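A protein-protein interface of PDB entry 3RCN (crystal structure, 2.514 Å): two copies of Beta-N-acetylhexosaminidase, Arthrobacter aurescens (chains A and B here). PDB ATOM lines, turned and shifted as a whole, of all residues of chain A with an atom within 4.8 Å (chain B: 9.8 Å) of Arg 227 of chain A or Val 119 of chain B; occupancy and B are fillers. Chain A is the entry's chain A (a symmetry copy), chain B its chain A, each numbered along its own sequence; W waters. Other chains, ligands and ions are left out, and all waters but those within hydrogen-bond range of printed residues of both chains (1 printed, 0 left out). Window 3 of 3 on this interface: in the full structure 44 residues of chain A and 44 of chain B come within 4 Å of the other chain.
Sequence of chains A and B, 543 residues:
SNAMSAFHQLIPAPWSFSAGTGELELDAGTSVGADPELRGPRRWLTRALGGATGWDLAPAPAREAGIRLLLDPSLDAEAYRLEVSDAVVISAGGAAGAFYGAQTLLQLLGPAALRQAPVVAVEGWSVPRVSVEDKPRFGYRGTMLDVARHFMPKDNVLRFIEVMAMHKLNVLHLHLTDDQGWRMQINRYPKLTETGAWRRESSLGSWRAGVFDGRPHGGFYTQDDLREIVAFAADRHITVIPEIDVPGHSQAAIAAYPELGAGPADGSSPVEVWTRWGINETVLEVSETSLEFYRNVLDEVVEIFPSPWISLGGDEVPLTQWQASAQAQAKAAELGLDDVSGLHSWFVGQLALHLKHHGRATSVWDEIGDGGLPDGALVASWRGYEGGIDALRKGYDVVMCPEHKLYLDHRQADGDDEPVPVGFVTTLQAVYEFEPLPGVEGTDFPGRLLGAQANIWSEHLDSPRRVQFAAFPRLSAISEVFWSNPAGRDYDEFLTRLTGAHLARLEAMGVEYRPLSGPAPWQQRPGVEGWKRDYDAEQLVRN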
ATOM      1  N   GLN A 223       5.859 -26.731 -10.680  1.00  0.00           N
ATOM      2  CA  GLN A 223       7.266 -26.415 -10.864  1.00  0.00           C
ATOM      3  C   GLN A 223       7.606 -26.548 -12.338  1.00  0.00           C
ATOM      4  O   GLN A 223       8.385 -25.763 -12.881  1.00  0.00           O
ATOM      5  CB  GLN A 223       8.147 -27.294  -9.976  1.00  0.00           C
ATOM      6  CG  GLN A 223       7.715 -27.264  -8.512  1.00  0.00           C
ATOM      7  CD  GLN A 223       8.887 -27.195  -7.526  1.00  0.00           C
ATOM      8  OE1 GLN A 223       9.958 -27.765  -7.761  1.00  0.00           O
ATOM      9  NE2 GLN A 223       8.680 -26.493  -6.418  1.00  0.00           N
ATOM     10  N   ASP A 224       6.981 -27.520 -12.990  1.00  0.00           N
ATOM     11  CA  ASP A 224       7.157 -27.707 -14.421  1.00  0.00           C
ATOM     12  C   ASP A 224       6.609 -26.534 -15.227  1.00  0.00           C
ATOM     13  O   ASP A 224       7.156 -26.185 -16.274  1.00  0.00           O
ATOM     14  CB  ASP A 224       6.520 -29.007 -14.867  1.00  0.00           C
ATOM     15  CG  ASP A 224       7.441 -30.184 -14.693  1.00  0.00           C
ATOM     16  OD1 ASP A 224       8.665 -29.950 -14.624  1.00  0.00           O
ATOM     17  OD2 ASP A 224       6.946 -31.337 -14.639  1.00  0.00           O
ATOM     18  N   ASP A 225       5.535 -25.927 -14.729  1.00  0.00           N
ATOM     19  CA  ASP A 225       4.949 -24.760 -15.370  1.00  0.00           C
ATOM     20  C   ASP A 225       5.899 -23.571 -15.263  1.00  0.00           C
ATOM     21  O   ASP A 225       6.088 -22.820 -16.225  1.00  0.00           O
ATOM     22  CB  ASP A 225       3.605 -24.398 -14.724  1.00  0.00           C
ATOM     23  CG  ASP A 225       2.525 -25.450 -14.956  1.00  0.00           C
ATOM     24  OD1 ASP A 225       1.637 -25.554 -14.080  1.00  0.00           O
ATOM     25  OD2 ASP A 225       2.545 -26.160 -15.997  1.00  0.00           O
ATOM     26  N   LEU A 226       6.489 -23.398 -14.083  1.00  0.00           N
ATOM     27  CA  LEU A 226       7.420 -22.304 -13.874  1.00  0.00           C
ATOM     28  C   LEU A 226       8.674 -22.509 -14.698  1.00  0.00           C
ATOM     29  O   LEU A 226       9.171 -21.583 -15.317  1.00  0.00           O
ATOM     30  CB  LEU A 226       7.755 -22.162 -12.394  1.00  0.00           C
ATOM     31  CG  LEU A 226       6.534 -21.754 -11.573  1.00  0.00           C
ATOM     32  CD1 LEU A 226       6.786 -21.921 -10.090  1.00  0.00           C
ATOM     33  CD2 LEU A 226       6.161 -20.339 -11.897  1.00  0.00           C
ATOM     34  N   ARG A 227       9.181 -23.732 -14.711  1.00  0.00           N
ATOM     35  CA  ARG A 227      10.339 -24.045 -15.531  1.00  0.00           C
ATOM     36  C   ARG A 227      10.066 -23.584 -16.957  1.00  0.00           C
ATOM     37  O   ARG A 227      10.842 -22.824 -17.531  1.00  0.00           O
ATOM     38  CB  ARG A 227      10.622 -25.543 -15.515  1.00  0.00           C
ATOM     39  CG  ARG A 227      11.145 -26.071 -14.209  1.00  0.00           C
ATOM     40  CD  ARG A 227      11.905 -27.393 -14.405  1.00  0.00           C
ATOM     41  NE  ARG A 227      12.514 -27.864 -13.158  1.00  0.00           N
ATOM     42  CZ  ARG A 227      11.880 -28.603 -12.247  1.00  0.00           C
ATOM     43  NH1 ARG A 227      10.615 -28.968 -12.448  1.00  0.00           N
ATOM     44  NH2 ARG A 227      12.503 -28.983 -11.136  1.00  0.00           N
ATOM     45  N   GLU A 228       8.946 -24.039 -17.511  1.00  0.00           N
ATOM     46  CA  GLU A 228       8.531 -23.663 -18.854  1.00  0.00           C
ATOM     47  C   GLU A 228       8.537 -22.147 -19.054  1.00  0.00           C
ATOM     48  O   GLU A 228       9.092 -21.633 -20.024  1.00  0.00           O
ATOM     49  CB  GLU A 228       7.149 -24.241 -19.169  1.00  0.00           C
ATOM     50  CG  GLU A 228       6.649 -23.945 -20.593  1.00  0.00           C
ATOM     51  CD  GLU A 228       5.304 -24.638 -20.939  1.00  0.00           C
ATOM     52  OE1 GLU A 228       4.611 -25.135 -20.027  1.00  0.00           O
ATOM     53  OE2 GLU A 228       4.931 -24.683 -22.136  1.00  0.00           O
ATOM     54  N   ILE A 229       7.926 -21.428 -18.128  1.00  0.00           N
ATOM     55  CA  ILE A 229       7.853 -19.988 -18.251  1.00  0.00           C
ATOM     56  C   ILE A 229       9.254 -19.384 -18.279  1.00  0.00           C
ATOM     57  O   ILE A 229       9.523 -18.471 -19.080  1.00  0.00           O
ATOM     58  CB  ILE A 229       7.058 -19.388 -17.101  1.00  0.00           C
ATOM     59  CG1 ILE A 229       5.566 -19.594 -17.341  1.00  0.00           C
ATOM     60  CG2 ILE A 229       7.373 -17.911 -16.968  1.00  0.00           C
ATOM     61  CD1 ILE A 229       4.717 -19.449 -16.103  1.00  0.00           C
ATOM     62  N   VAL A 230      10.137 -19.908 -17.412  1.00  0.00           N
ATOM     63  CA  VAL A 230      11.529 -19.478 -17.353  1.00  0.00           C
ATOM     64  C   VAL A 230      12.282 -19.787 -18.651  1.00  0.00           C
ATOM     65  O   VAL A 230      13.019 -18.944 -19.171  1.00  0.00           O
ATOM     66  CB  VAL A 230      12.294 -20.098 -16.137  1.00  0.00           C
ATOM     67  CG1 VAL A 230      13.787 -19.840 -16.258  1.00  0.00           C
ATOM     68  CG2 VAL A 230      11.777 -19.546 -14.812  1.00  0.00           C
ATOM     69  N   ALA A 231      12.105 -20.997 -19.171  1.00  0.00           N
ATOM     70  CA  ALA A 231      12.700 -21.372 -20.456  1.00  0.00           C
ATOM     71  C   ALA A 231      12.125 -20.554 -21.618  1.00  0.00           C
ATOM     72  O   ALA A 231      12.863 -20.111 -22.505  1.00  0.00           O
ATOM     73  CB  ALA A 231      12.527 -22.852 -20.710  1.00  0.00           C
ATOM     74  N   PHE A 232      10.810 -20.348 -21.601  1.00  0.00           N
ATOM     75  CA  PHE A 232      10.143 -19.545 -22.621  1.00  0.00           C
ATOM     76  C   PHE A 232      10.731 -18.132 -22.608  1.00  0.00           C
ATOM     77  O   PHE A 232      11.114 -17.600 -23.653  1.00  0.00           O
ATOM     78  CB  PHE A 232       8.619 -19.535 -22.375  1.00  0.00           C
ATOM     79  CG  PHE A 232       7.797 -18.970 -23.513  1.00  0.00           C
ATOM     80  CD1 PHE A 232       7.482 -17.620 -23.560  1.00  0.00           C
ATOM     81  CD2 PHE A 232       7.294 -19.794 -24.504  1.00  0.00           C
ATOM     82  CE1 PHE A 232       6.695 -17.102 -24.589  1.00  0.00           C
ATOM     83  CE2 PHE A 232       6.525 -19.277 -25.547  1.00  0.00           C
ATOM     84  CZ  PHE A 232       6.225 -17.934 -25.582  1.00  0.00           C
ATOM     85  N   ILE A 304      14.385 -23.576  -9.434  1.00  0.00           N
ATOM     86  CA  ILE A 304      13.542 -23.247 -10.583  1.00  0.00           C
ATOM     87  C   ILE A 304      13.999 -22.032 -11.406  1.00  0.00           C
ATOM     88  O   ILE A 304      14.079 -22.104 -12.633  1.00  0.00           O
ATOM     89  CB  ILE A 304      12.081 -22.992 -10.133  1.00  0.00           C
ATOM     90  CG1 ILE A 304      11.556 -24.158  -9.279  1.00  0.00           C
ATOM     91  CG2 ILE A 304      11.204 -22.705 -11.328  1.00  0.00           C
ATOM     92  CD1 ILE A 304      11.733 -25.513  -9.925  1.00  0.00           C
ATOM     93  N   LEU B  49       8.245 -29.409 -31.844  1.00  0.00           N
ATOM     94  CA  LEU B  49       9.274 -30.177 -31.170  1.00  0.00           C
ATOM     95  C   LEU B  49      10.541 -29.345 -30.960  1.00  0.00           C
ATOM     96  O   LEU B  49      11.223 -29.493 -29.952  1.00  0.00           O
ATOM     97  CB  LEU B  49       9.580 -31.434 -31.978  1.00  0.00           C
ATOM     98  CG  LEU B  49      10.463 -32.501 -31.347  1.00  0.00           C
ATOM     99  CD1 LEU B  49       9.824 -33.045 -30.073  1.00  0.00           C
ATOM    100  CD2 LEU B  49      10.685 -33.600 -32.354  1.00  0.00           C
ATOM    101  N   GLY B  50      10.856 -28.476 -31.913  1.00  0.00           N
ATOM    102  CA  GLY B  50      11.956 -27.547 -31.747  1.00  0.00           C
ATOM    103  C   GLY B  50      11.743 -26.663 -30.527  1.00  0.00           C
ATOM    104  O   GLY B  50      12.650 -26.460 -29.720  1.00  0.00           O
ATOM    105  N   GLY B  51      10.533 -26.140 -30.392  1.00  0.00           N
ATOM    106  CA  GLY B  51      10.181 -25.348 -29.238  1.00  0.00           C
ATOM    107  C   GLY B  51      10.349 -26.140 -27.952  1.00  0.00           C
ATOM    108  O   GLY B  51      10.835 -25.623 -26.944  1.00  0.00           O
ATOM    109  N   ALA B  52       9.952 -27.405 -27.969  1.00  0.00           N
ATOM    110  CA  ALA B  52      10.006 -28.170 -26.729  1.00  0.00           C
ATOM    111  C   ALA B  52      11.412 -28.657 -26.372  1.00  0.00           C
ATOM    112  O   ALA B  52      11.720 -28.806 -25.201  1.00  0.00           O
ATOM    113  CB  ALA B  52       9.016 -29.325 -26.754  1.00  0.00           C
ATOM    114  N   THR B  53      12.215 -28.995 -27.381  1.00  0.00           N
ATOM    115  CA  THR B  53      13.589 -29.445 -27.179  1.00  0.00           C
ATOM    116  C   THR B  53      14.734 -28.434 -27.301  1.00  0.00           C
ATOM    117  O   THR B  53      15.847 -28.731 -26.888  1.00  0.00           O
ATOM    118  CB  THR B  53      13.952 -30.533 -28.193  1.00  0.00           C
ATOM    119  OG1 THR B  53      14.055 -29.943 -29.498  1.00  0.00           O
ATOM    120  CG2 THR B  53      12.922 -31.651 -28.181  1.00  0.00           C
ATOM    121  N   GLY B  54      14.481 -27.247 -27.834  1.00  0.00           N
ATOM    122  CA  GLY B  54      15.581 -26.375 -28.217  1.00  0.00           C
ATOM    123  C   GLY B  54      16.451 -26.898 -29.368  1.00  0.00           C
ATOM    124  O   GLY B  54      17.500 -26.324 -29.667  1.00  0.00           O
ATOM    125  N   GLY B 110       6.669 -38.203 -24.491  1.00  0.00           N
ATOM    126  CA  GLY B 110       6.242 -37.786 -23.162  1.00  0.00           C
ATOM    127  C   GLY B 110       5.749 -36.348 -23.090  1.00  0.00           C
ATOM    128  O   GLY B 110       5.956 -35.580 -24.031  1.00  0.00           O
ATOM    129  N   PRO B 111       5.106 -35.973 -21.966  1.00  0.00           N
ATOM    130  CA  PRO B 111       4.457 -34.664 -21.808  1.00  0.00           C
ATOM    131  C   PRO B 111       5.375 -33.461 -22.030  1.00  0.00           C
ATOM    132  O   PRO B 111       4.858 -32.396 -22.387  1.00  0.00           O
ATOM    133  CB  PRO B 111       3.960 -34.686 -20.354  1.00  0.00           C
ATOM    134  CG  PRO B 111       3.816 -36.119 -20.032  1.00  0.00           C
ATOM    135  CD  PRO B 111       4.946 -36.796 -20.755  1.00  0.00           C
ATOM    136  N   ALA B 112       6.687 -33.603 -21.833  1.00  0.00           N
ATOM    137  CA  ALA B 112       7.570 -32.439 -21.996  1.00  0.00           C
ATOM    138  C   ALA B 112       7.660 -32.029 -23.463  1.00  0.00           C
ATOM    139  O   ALA B 112       8.035 -30.901 -23.795  1.00  0.00           O
ATOM    140  CB  ALA B 112       8.949 -32.701 -21.423  1.00  0.00           C
ATOM    141  N   ALA B 113       7.300 -32.959 -24.332  1.00  0.00           N
ATOM    142  CA  ALA B 113       7.259 -32.705 -25.762  1.00  0.00           C
ATOM    143  C   ALA B 113       6.120 -31.760 -26.155  1.00  0.00           C
ATOM    144  O   ALA B 113       6.129 -31.218 -27.255  1.00  0.00           O
ATOM    145  CB  ALA B 113       7.149 -34.012 -26.511  1.00  0.00           C
ATOM    146  N   LEU B 114       5.158 -31.555 -25.251  1.00  0.00           N
ATOM    147  CA  LEU B 114       4.032 -30.636 -25.481  1.00  0.00           C
ATOM    148  C   LEU B 114       4.207 -29.223 -24.924  1.00  0.00           C
ATOM    149  O   LEU B 114       3.329 -28.370 -25.091  1.00  0.00           O
ATOM    150  CB  LEU B 114       2.755 -31.225 -24.885  1.00  0.00           C
ATOM    151  CG  LEU B 114       2.453 -32.623 -25.407  1.00  0.00           C
ATOM    152  CD1 LEU B 114       1.294 -33.245 -24.660  1.00  0.00           C
ATOM    153  CD2 LEU B 114       2.170 -32.534 -26.888  1.00  0.00           C
ATOM    154  N   ARG B 115       5.318 -28.981 -24.233  1.00  0.00           N
ATOM    155  CA  ARG B 115       5.607 -27.648 -23.724  1.00  0.00           C
ATOM    156  C   ARG B 115       6.064 -26.727 -24.857  1.00  0.00           C
ATOM    157  O   ARG B 115       6.526 -27.189 -25.894  1.00  0.00           O
ATOM    158  CB  ARG B 115       6.668 -27.718 -22.624  1.00  0.00           C
ATOM    159  CG  ARG B 115       6.295 -28.626 -21.466  1.00  0.00           C
ATOM    160  CD  ARG B 115       5.418 -27.918 -20.450  1.00  0.00           C
ATOM    161  NE  ARG B 115       5.036 -28.801 -19.348  1.00  0.00           N
ATOM    162  CZ  ARG B 115       4.352 -28.403 -18.278  1.00  0.00           C
ATOM    163  NH1 ARG B 115       3.987 -27.134 -18.156  1.00  0.00           N
ATOM    164  NH2 ARG B 115       4.048 -29.271 -17.320  1.00  0.00           N
ATOM    165  N   GLN B 116       5.943 -25.423 -24.649  1.00  0.00           N
ATOM    166  CA  GLN B 116       6.380 -24.442 -25.639  1.00  0.00           C
ATOM    167  C   GLN B 116       7.841 -24.014 -25.443  1.00  0.00           C
ATOM    168  O   GLN B 116       8.386 -23.289 -26.262  1.00  0.00           O
ATOM    169  CB  GLN B 116       5.440 -23.225 -25.643  1.00  0.00           C
ATOM    170  CG  GLN B 116       3.963 -23.562 -25.966  1.00  0.00           C
ATOM    171  CD  GLN B 116       3.041 -22.337 -25.934  1.00  0.00           C
ATOM    172  OE1 GLN B 116       3.330 -21.299 -26.544  1.00  0.00           O
ATOM    173  NE2 GLN B 116       1.929 -22.452 -25.209  1.00  0.00           N
ATOM    174  N   ALA B 117       8.458 -24.448 -24.347  1.00  0.00           N
ATOM    175  CA  ALA B 117       9.903 -24.261 -24.108  1.00  0.00           C
ATOM    176  C   ALA B 117      10.435 -25.474 -23.347  1.00  0.00           C
ATOM    177  O   ALA B 117       9.668 -26.145 -22.663  1.00  0.00           O
ATOM    178  CB  ALA B 117      10.167 -22.976 -23.341  1.00  0.00           C
ATOM    179  N   PRO B 118      11.739 -25.780 -23.468  1.00  0.00           N
ATOM    180  CA  PRO B 118      12.178 -27.033 -22.822  1.00  0.00           C
ATOM    181  C   PRO B 118      12.089 -26.988 -21.299  1.00  0.00           C
ATOM    182  O   PRO B 118      12.597 -26.057 -20.686  1.00  0.00           O
ATOM    183  CB  PRO B 118      13.655 -27.143 -23.227  1.00  0.00           C
ATOM    184  CG  PRO B 118      13.844 -26.164 -24.358  1.00  0.00           C
ATOM    185  CD  PRO B 118      12.844 -25.071 -24.132  1.00  0.00           C
ATOM    186  N   VAL B 119      11.434 -27.975 -20.702  1.00  0.00           N
ATOM    187  CA  VAL B 119      11.459 -28.175 -19.256  1.00  0.00           C
ATOM    188  C   VAL B 119      12.413 -29.280 -18.793  1.00  0.00           C
ATOM    189  O   VAL B 119      12.426 -29.646 -17.617  1.00  0.00           O
ATOM    190  CB  VAL B 119      10.061 -28.344 -18.652  1.00  0.00           C
ATOM    191  CG1 VAL B 119       9.177 -27.153 -19.049  1.00  0.00           C
ATOM    192  CG2 VAL B 119       9.464 -29.679 -19.062  1.00  0.00           C
ATOM    193  N   VAL B 120      13.151 -29.866 -19.726  1.00  0.00           N
ATOM    194  CA  VAL B 120      14.046 -30.957 -19.365  1.00  0.00           C
ATOM    195  C   VAL B 120      15.490 -30.756 -19.836  1.00  0.00           C
ATOM    196  O   VAL B 120      15.822 -29.751 -20.461  1.00  0.00           O
ATOM    197  CB  VAL B 120      13.503 -32.314 -19.861  1.00  0.00           C
ATOM    198  CG1 VAL B 120      12.231 -32.674 -19.103  1.00  0.00           C
ATOM    199  CG2 VAL B 120      13.254 -32.277 -21.363  1.00  0.00           C
ATOM    200  N   ALA B 121      16.336 -31.734 -19.523  1.00  0.00           N
ATOM    201  CA  ALA B 121      17.774 -31.669 -19.785  1.00  0.00           C
ATOM    202  C   ALA B 121      18.124 -31.495 -21.265  1.00  0.00           C
ATOM    203  O   ALA B 121      19.024 -30.727 -21.608  1.00  0.00           O
ATOM    204  CB  ALA B 121      18.467 -32.910 -19.227  1.00  0.00           C
ATOM    205  N   VAL B 122      17.409 -32.210 -22.129  1.00  0.00           N
ATOM    206  CA  VAL B 122      17.640 -32.180 -23.569  1.00  0.00           C
ATOM    207  C   VAL B 122      18.998 -32.746 -24.015  1.00  0.00           C
ATOM    208  O   VAL B 122      19.434 -32.531 -25.151  1.00  0.00           O
ATOM    209  CB  VAL B 122      17.431 -30.725 -24.090  1.00  0.00           C
ATOM    210  CG1 VAL B 122      18.611 -30.219 -24.954  1.00  0.00           C
ATOM    211  CG2 VAL B 122      16.099 -30.613 -24.817  1.00  0.00           C
ATOM    212  N   GLU B 123      19.607 -33.571 -23.165  1.00  0.00           N
ATOM    213  CA  GLU B 123      20.848 -34.249 -23.547  1.00  0.00           C
ATOM    214  C   GLU B 123      20.474 -35.350 -24.523  1.00  0.00           C
ATOM    215  O   GLU B 123      21.061 -35.487 -25.602  1.00  0.00           O
ATOM    216  CB  GLU B 123      21.572 -34.824 -22.330  1.00  0.00           C
ATOM    217  CG  GLU B 123      22.007 -33.784 -21.306  1.00  0.00           C
ATOM    218  CD  GLU B 123      22.838 -32.663 -21.916  1.00  0.00           C
ATOM    219  OE1 GLU B 123      23.522 -32.906 -22.937  1.00  0.00           O
ATOM    220  OE2 GLU B 123      22.800 -31.534 -21.376  1.00  0.00           O
ATOM    221  N   TRP B 125      16.540 -37.527 -25.642  1.00  0.00           N
ATOM    222  CA  TRP B 125      15.188 -37.949 -25.365  1.00  0.00           C
ATOM    223  C   TRP B 125      15.123 -39.332 -25.929  1.00  0.00           C
ATOM    224  O   TRP B 125      15.917 -39.696 -26.791  1.00  0.00           O
ATOM    225  CB  TRP B 125      14.166 -37.076 -26.069  1.00  0.00           C
ATOM    226  CG  TRP B 125      14.129 -35.659 -25.638  1.00  0.00           C
ATOM    227  CD1 TRP B 125      15.188 -34.846 -25.408  1.00  0.00           C
ATOM    228  CD2 TRP B 125      12.956 -34.876 -25.386  1.00  0.00           C
ATOM    229  NE1 TRP B 125      14.754 -33.594 -25.029  1.00  0.00           N
ATOM    230  CE2 TRP B 125      13.385 -33.591 -25.003  1.00  0.00           C
ATOM    231  CE3 TRP B 125      11.585 -35.138 -25.445  1.00  0.00           C
ATOM    232  CZ2 TRP B 125      12.493 -32.566 -24.684  1.00  0.00           C
ATOM    233  CZ3 TRP B 125      10.702 -34.120 -25.128  1.00  0.00           C
ATOM    234  CH2 TRP B 125      11.158 -32.851 -24.756  1.00  0.00           C
ATOM    235  N   ALA B 504      -1.371 -35.660 -17.568  1.00  0.00           N
ATOM    236  CA  ALA B 504      -0.092 -34.946 -17.546  1.00  0.00           C
ATOM    237  C   ALA B 504       0.123 -34.180 -18.843  1.00  0.00           C
ATOM    238  O   ALA B 504       0.739 -33.110 -18.837  1.00  0.00           O
ATOM    239  CB  ALA B 504       1.059 -35.901 -17.308  1.00  0.00           C
ATOM    240  N   GLU B 507      -2.058 -31.095 -18.657  1.00  0.00           N
ATOM    241  CA  GLU B 507      -1.390 -30.126 -17.803  1.00  0.00           C
ATOM    242  C   GLU B 507      -0.301 -29.416 -18.586  1.00  0.00           C
ATOM    243  O   GLU B 507      -0.137 -28.210 -18.470  1.00  0.00           O
ATOM    244  CB  GLU B 507      -0.808 -30.781 -16.553  1.00  0.00           C
ATOM    245  CG  GLU B 507      -1.850 -31.165 -15.509  1.00  0.00           C
ATOM    246  CD  GLU B 507      -1.260 -31.968 -14.352  1.00  0.00           C
ATOM    247  OE1 GLU B 507      -0.106 -31.682 -13.928  1.00  0.00           O
ATOM    248  OE2 GLU B 507      -1.950 -32.894 -13.869  1.00  0.00           O
ATOM    249  N   ALA B 508       0.430 -30.165 -19.398  1.00  0.00           N
ATOM    250  CA  ALA B 508       1.533 -29.595 -20.150  1.00  0.00           C
ATOM    251  C   ALA B 508       1.053 -28.582 -21.203  1.00  0.00           C
ATOM    252  O   ALA B 508       1.789 -27.666 -21.572  1.00  0.00           O
ATOM    253  CB  ALA B 508       2.373 -30.710 -20.791  1.00  0.00           C
HETATM  254  O   HOH W   1      -0.392 -25.957 -16.951  1.00  0.00           O
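The guanidinium group of Arg 115 of chain B is in salt-bridge range of the side-chain carboxylate of Asp 225 of chain A, at 2.8 Å. OE1 of Glu 228 of chain A is in salt-bridge range of NH1 of Arg 115 of chain B, 2.8 Å away. The side-chain carboxylate (OE2) of Glu 228 of chain A lies within hydrogen-bond range of the backbone NH (N) of Gln 116 of chain B, 2.8 Å away.
Hydrophobic or aromatic side chains of chain B that line the printed part of chain A: Ala 117 and Val 119.
No position is printed for both chains. Of the 12 pairs that touch across the chains among the printed residues, none has its exchanged pair printed and touching as well.
Arg 115 of chain B touches Asp 224 of chain A. Asp 224 of chain A touches Val 119 of chain B. Val 119 of chain B touches Arg 227 of chain A (O to CD, 3.96 Å). O of Glu 228 of chain A touches CB of Ala 117 of chain B, at 3.7 Å. Val 119 of chain B touches Glu 228 of chain A. Ala 231 of chain A touches Ala 117 of chain B (CB to CB, 3.5 Å). Ala 231 of chain A touches Pro 118 of chain B. Phe 232 of chain A touches Gln 116 of chain B (CE2 to OE1, 3.9 Å). CB of Ala 117 of chain B touches N of Phe 232 of chain A, 3.2 Å away.
No residue of chain B comes within 4 Å of Leu 226 of chain A. Printed residues of chain B within 4 Å of Arg 227 of chain A: Val 119. Of the printed residues of chain B, Ala 231 of chain A touches Ala 117 and Pro 118. Printed residues of chain A within 4 Å of Ala 117 of chain B: Glu 228, Ala 231 and Phe 232. Of chain A, only Asp 224 (3.6 Å), Arg 227 (3.96 Å) and Glu 228 (3.5 Å) come within 4 Å of Val 119 of chain B. The nearest printed residue of chain A that does not touch Val 119 of chain B is Ala 231 of chain A (5.2 Å).
The side-chain carboxylate of Asp 224 of chain A lies within salt-bridge range of the guanidinium group of Arg 227 of chain A (3.1 Å).
Water W1 lies within hydrogen-bond range of the backbone carbonyl oxygen (O) of Glu 507 of chain B (2.7 Å) and the side-chain carboxylate (OD2) of Asp 225 of chain A (3.1 Å).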
